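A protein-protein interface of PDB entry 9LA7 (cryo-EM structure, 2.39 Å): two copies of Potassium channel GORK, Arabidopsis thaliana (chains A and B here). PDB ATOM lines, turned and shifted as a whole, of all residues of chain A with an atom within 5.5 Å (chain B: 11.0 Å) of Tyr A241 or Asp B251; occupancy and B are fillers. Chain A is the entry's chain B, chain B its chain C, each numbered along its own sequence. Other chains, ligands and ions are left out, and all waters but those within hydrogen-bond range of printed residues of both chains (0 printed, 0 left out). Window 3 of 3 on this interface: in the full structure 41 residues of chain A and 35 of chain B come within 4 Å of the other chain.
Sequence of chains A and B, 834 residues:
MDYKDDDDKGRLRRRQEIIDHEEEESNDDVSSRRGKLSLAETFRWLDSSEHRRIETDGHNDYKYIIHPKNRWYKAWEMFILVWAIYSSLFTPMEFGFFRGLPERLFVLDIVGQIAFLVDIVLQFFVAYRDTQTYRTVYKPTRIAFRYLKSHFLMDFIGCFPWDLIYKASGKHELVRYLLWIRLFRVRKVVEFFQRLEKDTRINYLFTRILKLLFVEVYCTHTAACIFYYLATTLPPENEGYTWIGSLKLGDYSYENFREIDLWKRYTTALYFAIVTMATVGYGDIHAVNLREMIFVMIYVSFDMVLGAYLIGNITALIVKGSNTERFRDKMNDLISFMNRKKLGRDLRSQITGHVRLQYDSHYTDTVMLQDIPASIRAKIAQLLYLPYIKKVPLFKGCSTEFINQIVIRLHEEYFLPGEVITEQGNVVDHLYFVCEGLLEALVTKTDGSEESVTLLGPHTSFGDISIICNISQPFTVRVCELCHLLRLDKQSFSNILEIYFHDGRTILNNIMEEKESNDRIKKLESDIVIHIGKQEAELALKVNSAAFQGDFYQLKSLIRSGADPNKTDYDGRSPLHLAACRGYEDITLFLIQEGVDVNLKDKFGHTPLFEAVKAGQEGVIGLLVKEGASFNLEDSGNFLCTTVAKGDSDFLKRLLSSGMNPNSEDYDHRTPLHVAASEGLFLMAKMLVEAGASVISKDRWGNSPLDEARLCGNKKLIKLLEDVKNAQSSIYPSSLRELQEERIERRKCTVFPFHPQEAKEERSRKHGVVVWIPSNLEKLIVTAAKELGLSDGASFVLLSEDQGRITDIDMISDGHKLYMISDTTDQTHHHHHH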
ATOM      1  N   LEU A 234       9.690 -10.591   9.051  1.00  0.00           N
ATOM      2  CA  LEU A 234      10.653  -9.528   9.262  1.00  0.00           C
ATOM      3  C   LEU A 234      12.071 -10.082   9.145  1.00  0.00           C
ATOM      4  O   LEU A 234      12.321 -11.245   9.474  1.00  0.00           O
ATOM      5  CB  LEU A 234      10.453  -8.884  10.630  1.00  0.00           C
ATOM      6  CG  LEU A 234       9.413  -7.766  10.703  1.00  0.00           C
ATOM      7  CD1 LEU A 234       9.650  -6.886  11.918  1.00  0.00           C
ATOM      8  CD2 LEU A 234       9.454  -6.937   9.436  1.00  0.00           C
ATOM      9  N   ASN A 238      15.749  -7.116  12.270  1.00  0.00           N
ATOM     10  CA  ASN A 238      14.577  -6.442  12.814  1.00  0.00           C
ATOM     11  C   ASN A 238      13.784  -7.348  13.749  1.00  0.00           C
ATOM     12  O   ASN A 238      12.642  -7.037  14.102  1.00  0.00           O
ATOM     13  CB  ASN A 238      13.687  -5.930  11.685  1.00  0.00           C
ATOM     14  CG  ASN A 238      14.250  -4.696  11.016  1.00  0.00           C
ATOM     15  OD1 ASN A 238      14.966  -4.787  10.021  1.00  0.00           O
ATOM     16  ND2 ASN A 238      13.932  -3.530  11.565  1.00  0.00           N
ATOM     17  N   GLU A 239      14.382  -8.468  14.156  1.00  0.00           N
ATOM     18  CA  GLU A 239      13.703  -9.435  15.007  1.00  0.00           C
ATOM     19  C   GLU A 239      13.318  -8.861  16.363  1.00  0.00           C
ATOM     20  O   GLU A 239      12.395  -9.378  16.998  1.00  0.00           O
ATOM     21  CB  GLU A 239      14.596 -10.657  15.177  1.00  0.00           C
ATOM     22  CG  GLU A 239      15.626 -10.503  16.266  1.00  0.00           C
ATOM     23  CD  GLU A 239      16.434 -11.752  16.463  1.00  0.00           C
ATOM     24  OE1 GLU A 239      17.440 -11.692  17.200  1.00  0.00           O
ATOM     25  OE2 GLU A 239      16.064 -12.796  15.887  1.00  0.00           O
ATOM     26  N   GLY A 240      13.992  -7.805  16.820  1.00  0.00           N
ATOM     27  CA  GLY A 240      13.590  -7.160  18.054  1.00  0.00           C
ATOM     28  C   GLY A 240      12.223  -6.518  17.977  1.00  0.00           C
ATOM     29  O   GLY A 240      11.627  -6.217  19.015  1.00  0.00           O
ATOM     30  N   TYR A 241      11.716  -6.295  16.767  1.00  0.00           N
ATOM     31  CA  TYR A 241      10.364  -5.792  16.593  1.00  0.00           C
ATOM     32  C   TYR A 241       9.325  -6.902  16.501  1.00  0.00           C
ATOM     33  O   TYR A 241       8.133  -6.610  16.561  1.00  0.00           O
ATOM     34  CB  TYR A 241      10.292  -4.901  15.349  1.00  0.00           C
ATOM     35  CG  TYR A 241       9.114  -3.951  15.334  1.00  0.00           C
ATOM     36  CD1 TYR A 241       8.492  -3.566  16.510  1.00  0.00           C
ATOM     37  CD2 TYR A 241       8.631  -3.431  14.141  1.00  0.00           C
ATOM     38  CE1 TYR A 241       7.411  -2.708  16.499  1.00  0.00           C
ATOM     39  CE2 TYR A 241       7.555  -2.566  14.121  1.00  0.00           C
ATOM     40  CZ  TYR A 241       6.952  -2.206  15.305  1.00  0.00           C
ATOM     41  OH  TYR A 241       5.879  -1.345  15.294  1.00  0.00           O
ATOM     42  N   THR A 242       9.730  -8.162  16.401  1.00  0.00           N
ATOM     43  CA  THR A 242       8.743  -9.224  16.306  1.00  0.00           C
ATOM     44  C   THR A 242       8.262  -9.640  17.696  1.00  0.00           C
ATOM     45  O   THR A 242       8.844  -9.280  18.722  1.00  0.00           O
ATOM     46  CB  THR A 242       9.311 -10.423  15.550  1.00  0.00           C
ATOM     47  OG1 THR A 242      10.362 -11.022  16.316  1.00  0.00           O
ATOM     48  CG2 THR A 242       9.855  -9.987  14.204  1.00  0.00           C
ATOM     49  N   TRP A 243       7.169 -10.406  17.717  1.00  0.00           N
ATOM     50  CA  TRP A 243       6.589 -10.835  18.985  1.00  0.00           C
ATOM     51  C   TRP A 243       7.485 -11.827  19.714  1.00  0.00           C
ATOM     52  O   TRP A 243       7.549 -11.808  20.947  1.00  0.00           O
ATOM     53  CB  TRP A 243       5.201 -11.441  18.757  1.00  0.00           C
ATOM     54  CG  TRP A 243       5.200 -12.732  17.990  1.00  0.00           C
ATOM     55  CD1 TRP A 243       5.057 -12.882  16.643  1.00  0.00           C
ATOM     56  CD2 TRP A 243       5.342 -14.053  18.526  1.00  0.00           C
ATOM     57  NE1 TRP A 243       5.103 -14.209  16.306  1.00  0.00           N
ATOM     58  CE2 TRP A 243       5.278 -14.951  17.443  1.00  0.00           C
ATOM     59  CE3 TRP A 243       5.518 -14.564  19.815  1.00  0.00           C
ATOM     60  CZ2 TRP A 243       5.384 -16.328  17.610  1.00  0.00           C
ATOM     61  CZ3 TRP A 243       5.624 -15.930  19.978  1.00  0.00           C
ATOM     62  CH2 TRP A 243       5.556 -16.797  18.881  1.00  0.00           C
ATOM     63  N   SER A 246      11.338 -10.299  20.597  1.00  0.00           N
ATOM     64  CA  SER A 246      11.389  -9.466  21.790  1.00  0.00           C
ATOM     65  C   SER A 246      10.915 -10.210  23.033  1.00  0.00           C
ATOM     66  O   SER A 246      10.835  -9.610  24.111  1.00  0.00           O
ATOM     67  CB  SER A 246      10.555  -8.197  21.585  1.00  0.00           C
ATOM     68  OG  SER A 246       9.224  -8.516  21.226  1.00  0.00           O
ATOM     69  N   VAL A 288       3.430  -7.256  18.340  1.00  0.00           N
ATOM     70  CA  VAL A 288       4.325  -6.109  18.405  1.00  0.00           C
ATOM     71  C   VAL A 288       4.337  -5.317  17.102  1.00  0.00           C
ATOM     72  O   VAL A 288       4.096  -4.104  17.112  1.00  0.00           O
ATOM     73  CB  VAL A 288       5.756  -6.537  18.794  1.00  0.00           C
ATOM     74  CG1 VAL A 288       6.664  -5.338  18.801  1.00  0.00           C
ATOM     75  CG2 VAL A 288       5.769  -7.228  20.144  1.00  0.00           C
ATOM     76  N   ASN A 289       4.621  -5.968  15.967  1.00  0.00           N
ATOM     77  CA  ASN A 289       4.479  -5.334  14.658  1.00  0.00           C
ATOM     78  C   ASN A 289       3.022  -4.978  14.395  1.00  0.00           C
ATOM     79  O   ASN A 289       2.109  -5.469  15.059  1.00  0.00           O
ATOM     80  CB  ASN A 289       4.968  -6.235  13.526  1.00  0.00           C
ATOM     81  CG  ASN A 289       6.238  -6.954  13.842  1.00  0.00           C
ATOM     82  OD1 ASN A 289       7.198  -6.344  14.286  1.00  0.00           O
ATOM     83  ND2 ASN A 289       6.275  -8.251  13.567  1.00  0.00           N
ATOM     84  N   LEU A 290       2.792  -4.143  13.381  1.00  0.00           N
ATOM     85  CA  LEU A 290       1.452  -3.897  12.867  1.00  0.00           C
ATOM     86  C   LEU A 290       0.835  -5.132  12.230  1.00  0.00           C
ATOM     87  O   LEU A 290      -0.369  -5.357  12.383  1.00  0.00           O
ATOM     88  CB  LEU A 290       1.468  -2.772  11.830  1.00  0.00           C
ATOM     89  CG  LEU A 290       1.581  -1.324  12.300  1.00  0.00           C
ATOM     90  CD1 LEU A 290       0.939  -0.425  11.263  1.00  0.00           C
ATOM     91  CD2 LEU A 290       0.943  -1.137  13.661  1.00  0.00           C
ATOM     92  N   GLU A 292       1.437  -8.182  13.154  1.00  0.00           N
ATOM     93  CA  GLU A 292       1.019  -8.964  14.307  1.00  0.00           C
ATOM     94  C   GLU A 292      -0.283  -8.442  14.900  1.00  0.00           C
ATOM     95  O   GLU A 292      -1.162  -9.239  15.240  1.00  0.00           O
ATOM     96  CB  GLU A 292       2.121  -8.977  15.362  1.00  0.00           C
ATOM     97  CG  GLU A 292       3.102 -10.116  15.222  1.00  0.00           C
ATOM     98  CD  GLU A 292       4.520  -9.687  15.494  1.00  0.00           C
ATOM     99  OE1 GLU A 292       4.741  -8.956  16.479  1.00  0.00           O
ATOM    100  OE2 GLU A 292       5.422 -10.080  14.723  1.00  0.00           O
ATOM    101  N   ILE B 244      -0.696   5.712  24.735  1.00  0.00           N
ATOM    102  CA  ILE B 244       0.159   5.511  23.572  1.00  0.00           C
ATOM    103  C   ILE B 244       1.503   6.209  23.741  1.00  0.00           C
ATOM    104  O   ILE B 244       2.531   5.698  23.297  1.00  0.00           O
ATOM    105  CB  ILE B 244      -0.574   5.978  22.296  1.00  0.00           C
ATOM    106  CG1 ILE B 244       0.295   5.768  21.058  1.00  0.00           C
ATOM    107  CG2 ILE B 244      -0.996   7.424  22.412  1.00  0.00           C
ATOM    108  CD1 ILE B 244      -0.495   5.596  19.786  1.00  0.00           C
ATOM    109  N   SER B 246       3.204   6.531  26.430  1.00  0.00           N
ATOM    110  CA  SER B 246       4.007   5.695  27.309  1.00  0.00           C
ATOM    111  C   SER B 246       4.156   4.277  26.782  1.00  0.00           C
ATOM    112  O   SER B 246       4.762   3.436  27.452  1.00  0.00           O
ATOM    113  CB  SER B 246       3.395   5.664  28.709  1.00  0.00           C
ATOM    114  OG  SER B 246       1.997   5.457  28.646  1.00  0.00           O
ATOM    115  N   LEU B 247       3.625   3.996  25.598  1.00  0.00           N
ATOM    116  CA  LEU B 247       3.575   2.642  25.066  1.00  0.00           C
ATOM    117  C   LEU B 247       4.915   2.278  24.441  1.00  0.00           C
ATOM    118  O   LEU B 247       5.513   3.083  23.721  1.00  0.00           O
ATOM    119  CB  LEU B 247       2.450   2.518  24.043  1.00  0.00           C
ATOM    120  CG  LEU B 247       2.371   1.208  23.268  1.00  0.00           C
ATOM    121  CD1 LEU B 247       2.049   0.066  24.203  1.00  0.00           C
ATOM    122  CD2 LEU B 247       1.320   1.325  22.196  1.00  0.00           C
ATOM    123  N   LYS B 248       5.383   1.068  24.726  1.00  0.00           N
ATOM    124  CA  LYS B 248       6.614   0.528  24.160  1.00  0.00           C
ATOM    125  C   LYS B 248       6.343  -0.932  23.813  1.00  0.00           C
ATOM    126  O   LYS B 248       6.112  -1.756  24.702  1.00  0.00           O
ATOM    127  CB  LYS B 248       7.776   0.672  25.136  1.00  0.00           C
ATOM    128  CG  LYS B 248       9.111   0.951  24.479  1.00  0.00           C
ATOM    129  CD  LYS B 248       9.766  -0.320  23.979  1.00  0.00           C
ATOM    130  CE  LYS B 248      11.271  -0.274  24.178  1.00  0.00           C
ATOM    131  NZ  LYS B 248      11.907   0.769  23.329  1.00  0.00           N
ATOM    132  N   LEU B 249       6.362  -1.248  22.524  1.00  0.00           N
ATOM    133  CA  LEU B 249       6.102  -2.597  22.042  1.00  0.00           C
ATOM    134  C   LEU B 249       7.330  -3.101  21.301  1.00  0.00           C
ATOM    135  O   LEU B 249       7.696  -2.553  20.257  1.00  0.00           O
ATOM    136  CB  LEU B 249       4.869  -2.617  21.139  1.00  0.00           C
ATOM    137  CG  LEU B 249       3.547  -2.522  21.899  1.00  0.00           C
ATOM    138  CD1 LEU B 249       2.380  -2.717  20.971  1.00  0.00           C
ATOM    139  CD2 LEU B 249       3.507  -3.551  23.012  1.00  0.00           C
ATOM    140  N   GLY B 250       7.956  -4.147  21.834  1.00  0.00           N
ATOM    141  CA  GLY B 250       9.212  -4.629  21.295  1.00  0.00           C
ATOM    142  C   GLY B 250      10.284  -3.563  21.330  1.00  0.00           C
ATOM    143  O   GLY B 250      10.516  -2.945  22.372  1.00  0.00           O
ATOM    144  N   ASP B 251      10.953  -3.340  20.201  1.00  0.00           N
ATOM    145  CA  ASP B 251      11.901  -2.241  20.068  1.00  0.00           C
ATOM    146  C   ASP B 251      11.226  -0.888  19.928  1.00  0.00           C
ATOM    147  O   ASP B 251      11.734   0.108  20.451  1.00  0.00           O
ATOM    148  CB  ASP B 251      12.815  -2.463  18.858  1.00  0.00           C
ATOM    149  CG  ASP B 251      13.766  -3.616  19.051  1.00  0.00           C
ATOM    150  OD1 ASP B 251      13.897  -4.097  20.196  1.00  0.00           O
ATOM    151  OD2 ASP B 251      14.396  -4.033  18.058  1.00  0.00           O
ATOM    152  N   TYR B 252      10.093  -0.830  19.233  1.00  0.00           N
ATOM    153  CA  TYR B 252       9.464   0.444  18.911  1.00  0.00           C
ATOM    154  C   TYR B 252       8.898   1.096  20.164  1.00  0.00           C
ATOM    155  O   TYR B 252       8.223   0.444  20.966  1.00  0.00           O
ATOM    156  CB  TYR B 252       8.362   0.243  17.877  1.00  0.00           C
ATOM    157  CG  TYR B 252       7.865   1.532  17.269  1.00  0.00           C
ATOM    158  CD1 TYR B 252       8.604   2.191  16.301  1.00  0.00           C
ATOM    159  CD2 TYR B 252       6.659   2.091  17.667  1.00  0.00           C
ATOM    160  CE1 TYR B 252       8.162   3.368  15.745  1.00  0.00           C
ATOM    161  CE2 TYR B 252       6.206   3.270  17.115  1.00  0.00           C
ATOM    162  CZ  TYR B 252       6.962   3.903  16.153  1.00  0.00           C
ATOM    163  OH  TYR B 252       6.522   5.079  15.593  1.00  0.00           O
ATOM    164  N   SER B 253       9.177   2.382  20.329  1.00  0.00           N
ATOM    165  CA  SER B 253       8.570   3.192  21.373  1.00  0.00           C
ATOM    166  C   SER B 253       7.707   4.256  20.709  1.00  0.00           C
ATOM    167  O   SER B 253       8.189   5.006  19.856  1.00  0.00           O
ATOM    168  CB  SER B 253       9.635   3.831  22.260  1.00  0.00           C
ATOM    169  OG  SER B 253       9.130   4.990  22.893  1.00  0.00           O
ATOM    170  N   TYR B 254       6.437   4.313  21.096  1.00  0.00           N
ATOM    171  CA  TYR B 254       5.525   5.307  20.547  1.00  0.00           C
ATOM    172  C   TYR B 254       5.762   6.655  21.210  1.00  0.00           C
ATOM    173  O   TYR B 254       4.850   7.203  21.836  1.00  0.00           O
ATOM    174  CB  TYR B 254       4.067   4.885  20.749  1.00  0.00           C
ATOM    175  CG  TYR B 254       3.623   3.657  19.985  1.00  0.00           C
ATOM    176  CD1 TYR B 254       4.167   2.408  20.252  1.00  0.00           C
ATOM    177  CD2 TYR B 254       2.639   3.746  19.013  1.00  0.00           C
ATOM    178  CE1 TYR B 254       3.755   1.289  19.559  1.00  0.00           C
ATOM    179  CE2 TYR B 254       2.222   2.634  18.317  1.00  0.00           C
ATOM    180  CZ  TYR B 254       2.781   1.409  18.594  1.00  0.00           C
ATOM    181  OH  TYR B 254       2.363   0.303  17.900  1.00  0.00           O
ATOM    182  N   GLU B 255       6.970   7.207  21.084  1.00  0.00           N
ATOM    183  CA  GLU B 255       7.289   8.402  21.855  1.00  0.00           C
ATOM    184  C   GLU B 255       6.523   9.609  21.337  1.00  0.00           C
ATOM    185  O   GLU B 255       5.537  10.030  21.942  1.00  0.00           O
ATOM    186  CB  GLU B 255       8.794   8.672  21.804  1.00  0.00           C
ATOM    187  CG  GLU B 255       9.586   8.076  22.946  1.00  0.00           C
ATOM    188  CD  GLU B 255      11.039   7.845  22.579  1.00  0.00           C
ATOM    189  OE1 GLU B 255      11.500   8.433  21.577  1.00  0.00           O
ATOM    190  OE2 GLU B 255      11.720   7.077  23.288  1.00  0.00           O
ATOM    191  N   ILE B 260       3.570   9.895  14.503  1.00  0.00           N
ATOM    192  CA  ILE B 260       3.623   8.538  13.975  1.00  0.00           C
ATOM    193  C   ILE B 260       2.645   8.450  12.812  1.00  0.00           C
ATOM    194  O   ILE B 260       1.675   9.210  12.739  1.00  0.00           O
ATOM    195  CB  ILE B 260       3.314   7.505  15.082  1.00  0.00           C
ATOM    196  CG1 ILE B 260       4.337   7.616  16.212  1.00  0.00           C
ATOM    197  CG2 ILE B 260       3.325   6.086  14.547  1.00  0.00           C
ATOM    198  CD1 ILE B 260       4.166   6.565  17.286  1.00  0.00           C
ATOM    199  N   ASP B 261       2.914   7.535  11.881  1.00  0.00           N
ATOM    200  CA  ASP B 261       2.040   7.340  10.733  1.00  0.00           C
ATOM    201  C   ASP B 261       0.616   7.067  11.193  1.00  0.00           C
ATOM    202  O   ASP B 261       0.390   6.382  12.193  1.00  0.00           O
ATOM    203  CB  ASP B 261       2.549   6.182   9.872  1.00  0.00           C
ATOM    204  CG  ASP B 261       1.566   5.786   8.785  1.00  0.00           C
ATOM    205  OD1 ASP B 261       1.122   6.671   8.026  1.00  0.00           O
ATOM    206  OD2 ASP B 261       1.238   4.585   8.690  1.00  0.00           O
ATOM    207  N   TRP B 263      -1.760   5.202  10.109  1.00  0.00           N
ATOM    208  CA  TRP B 263      -2.207   3.820  10.173  1.00  0.00           C
ATOM    209  C   TRP B 263      -1.522   3.034  11.278  1.00  0.00           C
ATOM    210  O   TRP B 263      -2.140   2.124  11.828  1.00  0.00           O
ATOM    211  CB  TRP B 263      -2.020   3.150   8.817  1.00  0.00           C
ATOM    212  CG  TRP B 263      -2.904   3.769   7.788  1.00  0.00           C
ATOM    213  CD1 TRP B 263      -2.523   4.530   6.728  1.00  0.00           C
ATOM    214  CD2 TRP B 263      -4.335   3.718   7.753  1.00  0.00           C
ATOM    215  NE1 TRP B 263      -3.624   4.941   6.019  1.00  0.00           N
ATOM    216  CE2 TRP B 263      -4.750   4.456   6.630  1.00  0.00           C
ATOM    217  CE3 TRP B 263      -5.304   3.112   8.557  1.00  0.00           C
ATOM    218  CZ2 TRP B 263      -6.091   4.603   6.289  1.00  0.00           C
ATOM    219  CZ3 TRP B 263      -6.633   3.259   8.218  1.00  0.00           C
ATOM    220  CH2 TRP B 263      -7.014   3.999   7.094  1.00  0.00           C
ATOM    221  N   LYS B 264      -0.285   3.377  11.646  1.00  0.00           N
ATOM    222  CA  LYS B 264       0.306   2.770  12.838  1.00  0.00           C
ATOM    223  C   LYS B 264      -0.510   3.096  14.080  1.00  0.00           C
ATOM    224  O   LYS B 264      -0.836   2.204  14.873  1.00  0.00           O
ATOM    225  CB  LYS B 264       1.745   3.242  13.023  1.00  0.00           C
ATOM    226  CG  LYS B 264       2.783   2.358  12.380  1.00  0.00           C
ATOM    227  CD  LYS B 264       4.039   2.291  13.223  1.00  0.00           C
ATOM    228  CE  LYS B 264       3.867   1.302  14.356  1.00  0.00           C
ATOM    229  NZ  LYS B 264       5.152   1.029  15.043  1.00  0.00           N
ATOM    230  N   ARG B 265      -0.854   4.373  14.258  1.00  0.00           N
ATOM    231  CA  ARG B 265      -1.648   4.798  15.401  1.00  0.00           C
ATOM    232  C   ARG B 265      -3.019   4.141  15.406  1.00  0.00           C
ATOM    233  O   ARG B 265      -3.479   3.659  16.449  1.00  0.00           O
ATOM    234  CB  ARG B 265      -1.799   6.316  15.384  1.00  0.00           C
ATOM    235  CG  ARG B 265      -0.559   7.065  15.792  1.00  0.00           C
ATOM    236  CD  ARG B 265      -0.743   8.551  15.596  1.00  0.00           C
ATOM    237  NE  ARG B 265      -0.792   8.962  14.199  1.00  0.00           N
ATOM    238  CZ  ARG B 265      -1.493   9.994  13.754  1.00  0.00           C
ATOM    239  NH1 ARG B 265      -2.273  10.696  14.558  1.00  0.00           N
ATOM    240  NH2 ARG B 265      -1.412  10.330  12.471  1.00  0.00           N
ATOM    241  N   THR B 267      -3.933   1.348  13.880  1.00  0.00           N
ATOM    242  CA  THR B 267      -3.802  -0.085  14.091  1.00  0.00           C
ATOM    243  C   THR B 267      -3.541  -0.398  15.553  1.00  0.00           C
ATOM    244  O   THR B 267      -4.081  -1.365  16.086  1.00  0.00           O
ATOM    245  CB  THR B 267      -2.688  -0.650  13.210  1.00  0.00           C
ATOM    246  OG1 THR B 267      -2.811  -0.116  11.887  1.00  0.00           O
ATOM    247  CG2 THR B 267      -2.775  -2.163  13.149  1.00  0.00           C
ATOM    248  N   THR B 268      -2.729   0.419  16.225  1.00  0.00           N
ATOM    249  CA  THR B 268      -2.493   0.203  17.649  1.00  0.00           C
ATOM    250  C   THR B 268      -3.765   0.415  18.464  1.00  0.00           C
ATOM    251  O   THR B 268      -4.104  -0.402  19.334  1.00  0.00           O
ATOM    252  CB  THR B 268      -1.383   1.131  18.136  1.00  0.00           C
ATOM    253  OG1 THR B 268      -0.230   0.969  17.303  1.00  0.00           O
ATOM    254  CG2 THR B 268      -1.010   0.803  19.561  1.00  0.00           C
ATOM    255  N   TYR B 271      -6.141  -2.367  17.704  1.00  0.00           N
ATOM    256  CA  TYR B 271      -5.665  -3.583  18.342  1.00  0.00           C
ATOM    257  C   TYR B 271      -6.070  -3.614  19.806  1.00  0.00           C
ATOM    258  O   TYR B 271      -6.599  -4.621  20.290  1.00  0.00           O
ATOM    259  CB  TYR B 271      -4.149  -3.673  18.181  1.00  0.00           C
ATOM    260  CG  TYR B 271      -3.465  -4.736  19.001  1.00  0.00           C
ATOM    261  CD1 TYR B 271      -3.653  -6.081  18.724  1.00  0.00           C
ATOM    262  CD2 TYR B 271      -2.607  -4.394  20.031  1.00  0.00           C
ATOM    263  CE1 TYR B 271      -3.017  -7.051  19.462  1.00  0.00           C
ATOM    264  CE2 TYR B 271      -1.967  -5.359  20.774  1.00  0.00           C
ATOM    265  CZ  TYR B 271      -2.175  -6.687  20.486  1.00  0.00           C
ATOM    266  OH  TYR B 271      -1.538  -7.652  21.226  1.00  0.00           O
ATOM    267  N   ASP B 284      -0.258  -5.221  27.148  1.00  0.00           N
ATOM    268  CA  ASP B 284       0.696  -4.450  26.358  1.00  0.00           C
ATOM    269  C   ASP B 284       0.206  -3.021  26.165  1.00  0.00           C
ATOM    270  O   ASP B 284       0.966  -2.061  26.330  1.00  0.00           O
ATOM    271  CB  ASP B 284       0.944  -5.136  25.013  1.00  0.00           C
ATOM    272  CG  ASP B 284      -0.330  -5.626  24.361  1.00  0.00           C
ATOM    273  OD1 ASP B 284      -1.416  -5.425  24.939  1.00  0.00           O
ATOM    274  OD2 ASP B 284      -0.246  -6.214  23.265  1.00  0.00           O
ATOM    275  N   ILE B 285      -1.070  -2.861  25.830  1.00  0.00           N
ATOM    276  CA  ILE B 285      -1.720  -1.556  25.787  1.00  0.00           C
ATOM    277  C   ILE B 285      -2.807  -1.536  26.848  1.00  0.00           C
ATOM    278  O   ILE B 285      -3.628  -2.457  26.925  1.00  0.00           O
ATOM    279  CB  ILE B 285      -2.306  -1.256  24.396  1.00  0.00           C
ATOM    280  CG1 ILE B 285      -1.202  -1.150  23.348  1.00  0.00           C
ATOM    281  CG2 ILE B 285      -3.073   0.044  24.429  1.00  0.00           C
ATOM    282  CD1 ILE B 285      -1.042  -2.375  22.501  1.00  0.00           C
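NZ of Lys B264 sits at hydrogen-bond distance from OH of Tyr A241, at 2.5 Å. The backbone NH (N) of Asp B251 is in hydrogen-bond range of the backbone carbonyl oxygen (O) of Gly A240 (3.2 Å).
O of Tyr A241 lies close to OD1 of Asn A289, 2.5 Å away. The side-chain hydroxyl of Thr B268 is in hydrogen-bond range of the backbone carbonyl oxygen of Lys B264, 2.8 Å away. The backbone carbonyl oxygen (O) of Asp B251 lies within hydrogen-bond range of the side-chain amino group (NZ) of Lys B248. The backbone carbonyl oxygen of Thr A242 lies within hydrogen-bond range of the side-chain hydroxyl of Ser A246, at 2.6 Å. The backbone NH (N) of Val A288 sits at hydrogen-bond distance from the side-chain carboxylate (OE1) of Glu A292 (2.8 Å).
Among the printed residues, merely in contact across the chains: Gly A240 with Gly B250, Tyr A241 with Leu B249, Tyr A241 with Asp B251, Tyr A241 with Tyr B252, Ser A246 with Gly B250, Val A288 with Leu B249, Val A288 with Gly B250, Leu A290 with Lys B264 and Leu A290 with Thr B267.
Tyr A241 touches just these residues of chain B: Leu B249, Asp B251, Tyr B252 and Lys B264. Printed residues of chain A within 4 Å of Asp B251: Gly A240 and Tyr A241. Gly A240 touches two residues of chain B. Thr A242 touches none of the printed residues of chain B. Of the printed residues of chain B, Val A288 touches Leu B249 and Gly B250. No residue of chain B comes within 4 Å of Asn A289. Of the printed residues of chain A, Tyr B252 touches Tyr A241 (3.4 Å). Of the printed residues of chain B, Ser A246 touches Gly B250 (3.8 Å). Of the printed residues of chain A, Leu B249 touches Tyr A241 and Val A288. Of the printed residues of chain A, Thr B267 touches Leu A290. Ile B260 touches none of the printed residues of chain A. Thr B268 touches none of the printed residues of chain A. The nearest residue of chain B that does not touch Tyr A241 is Tyr B254 (4.7 Å). The nearest residue of chain A that does not touch Asp B251 is Val A288 (4.9 Å).
Printed residues of chain B that touch a printed residue of chain A: Leu B249, Gly B250, Asp B251, Tyr B252, Lys B264 and Thr B267. Hydrophobic or aromatic side chains of chain B that line the printed part of chain A: Tyr B252. Hydrophobic or aromatic side chains of chain A that line the printed part of chain B: Tyr A241, Val A288 and Leu A290. Among the printed residues, 11 pairs touch across the chains. Among the printed residues, no Asp or Glu carboxylate lies within 4 Å of a Lys or Arg side-chain nitrogen of the other chain.
1 position is printed for both chains.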
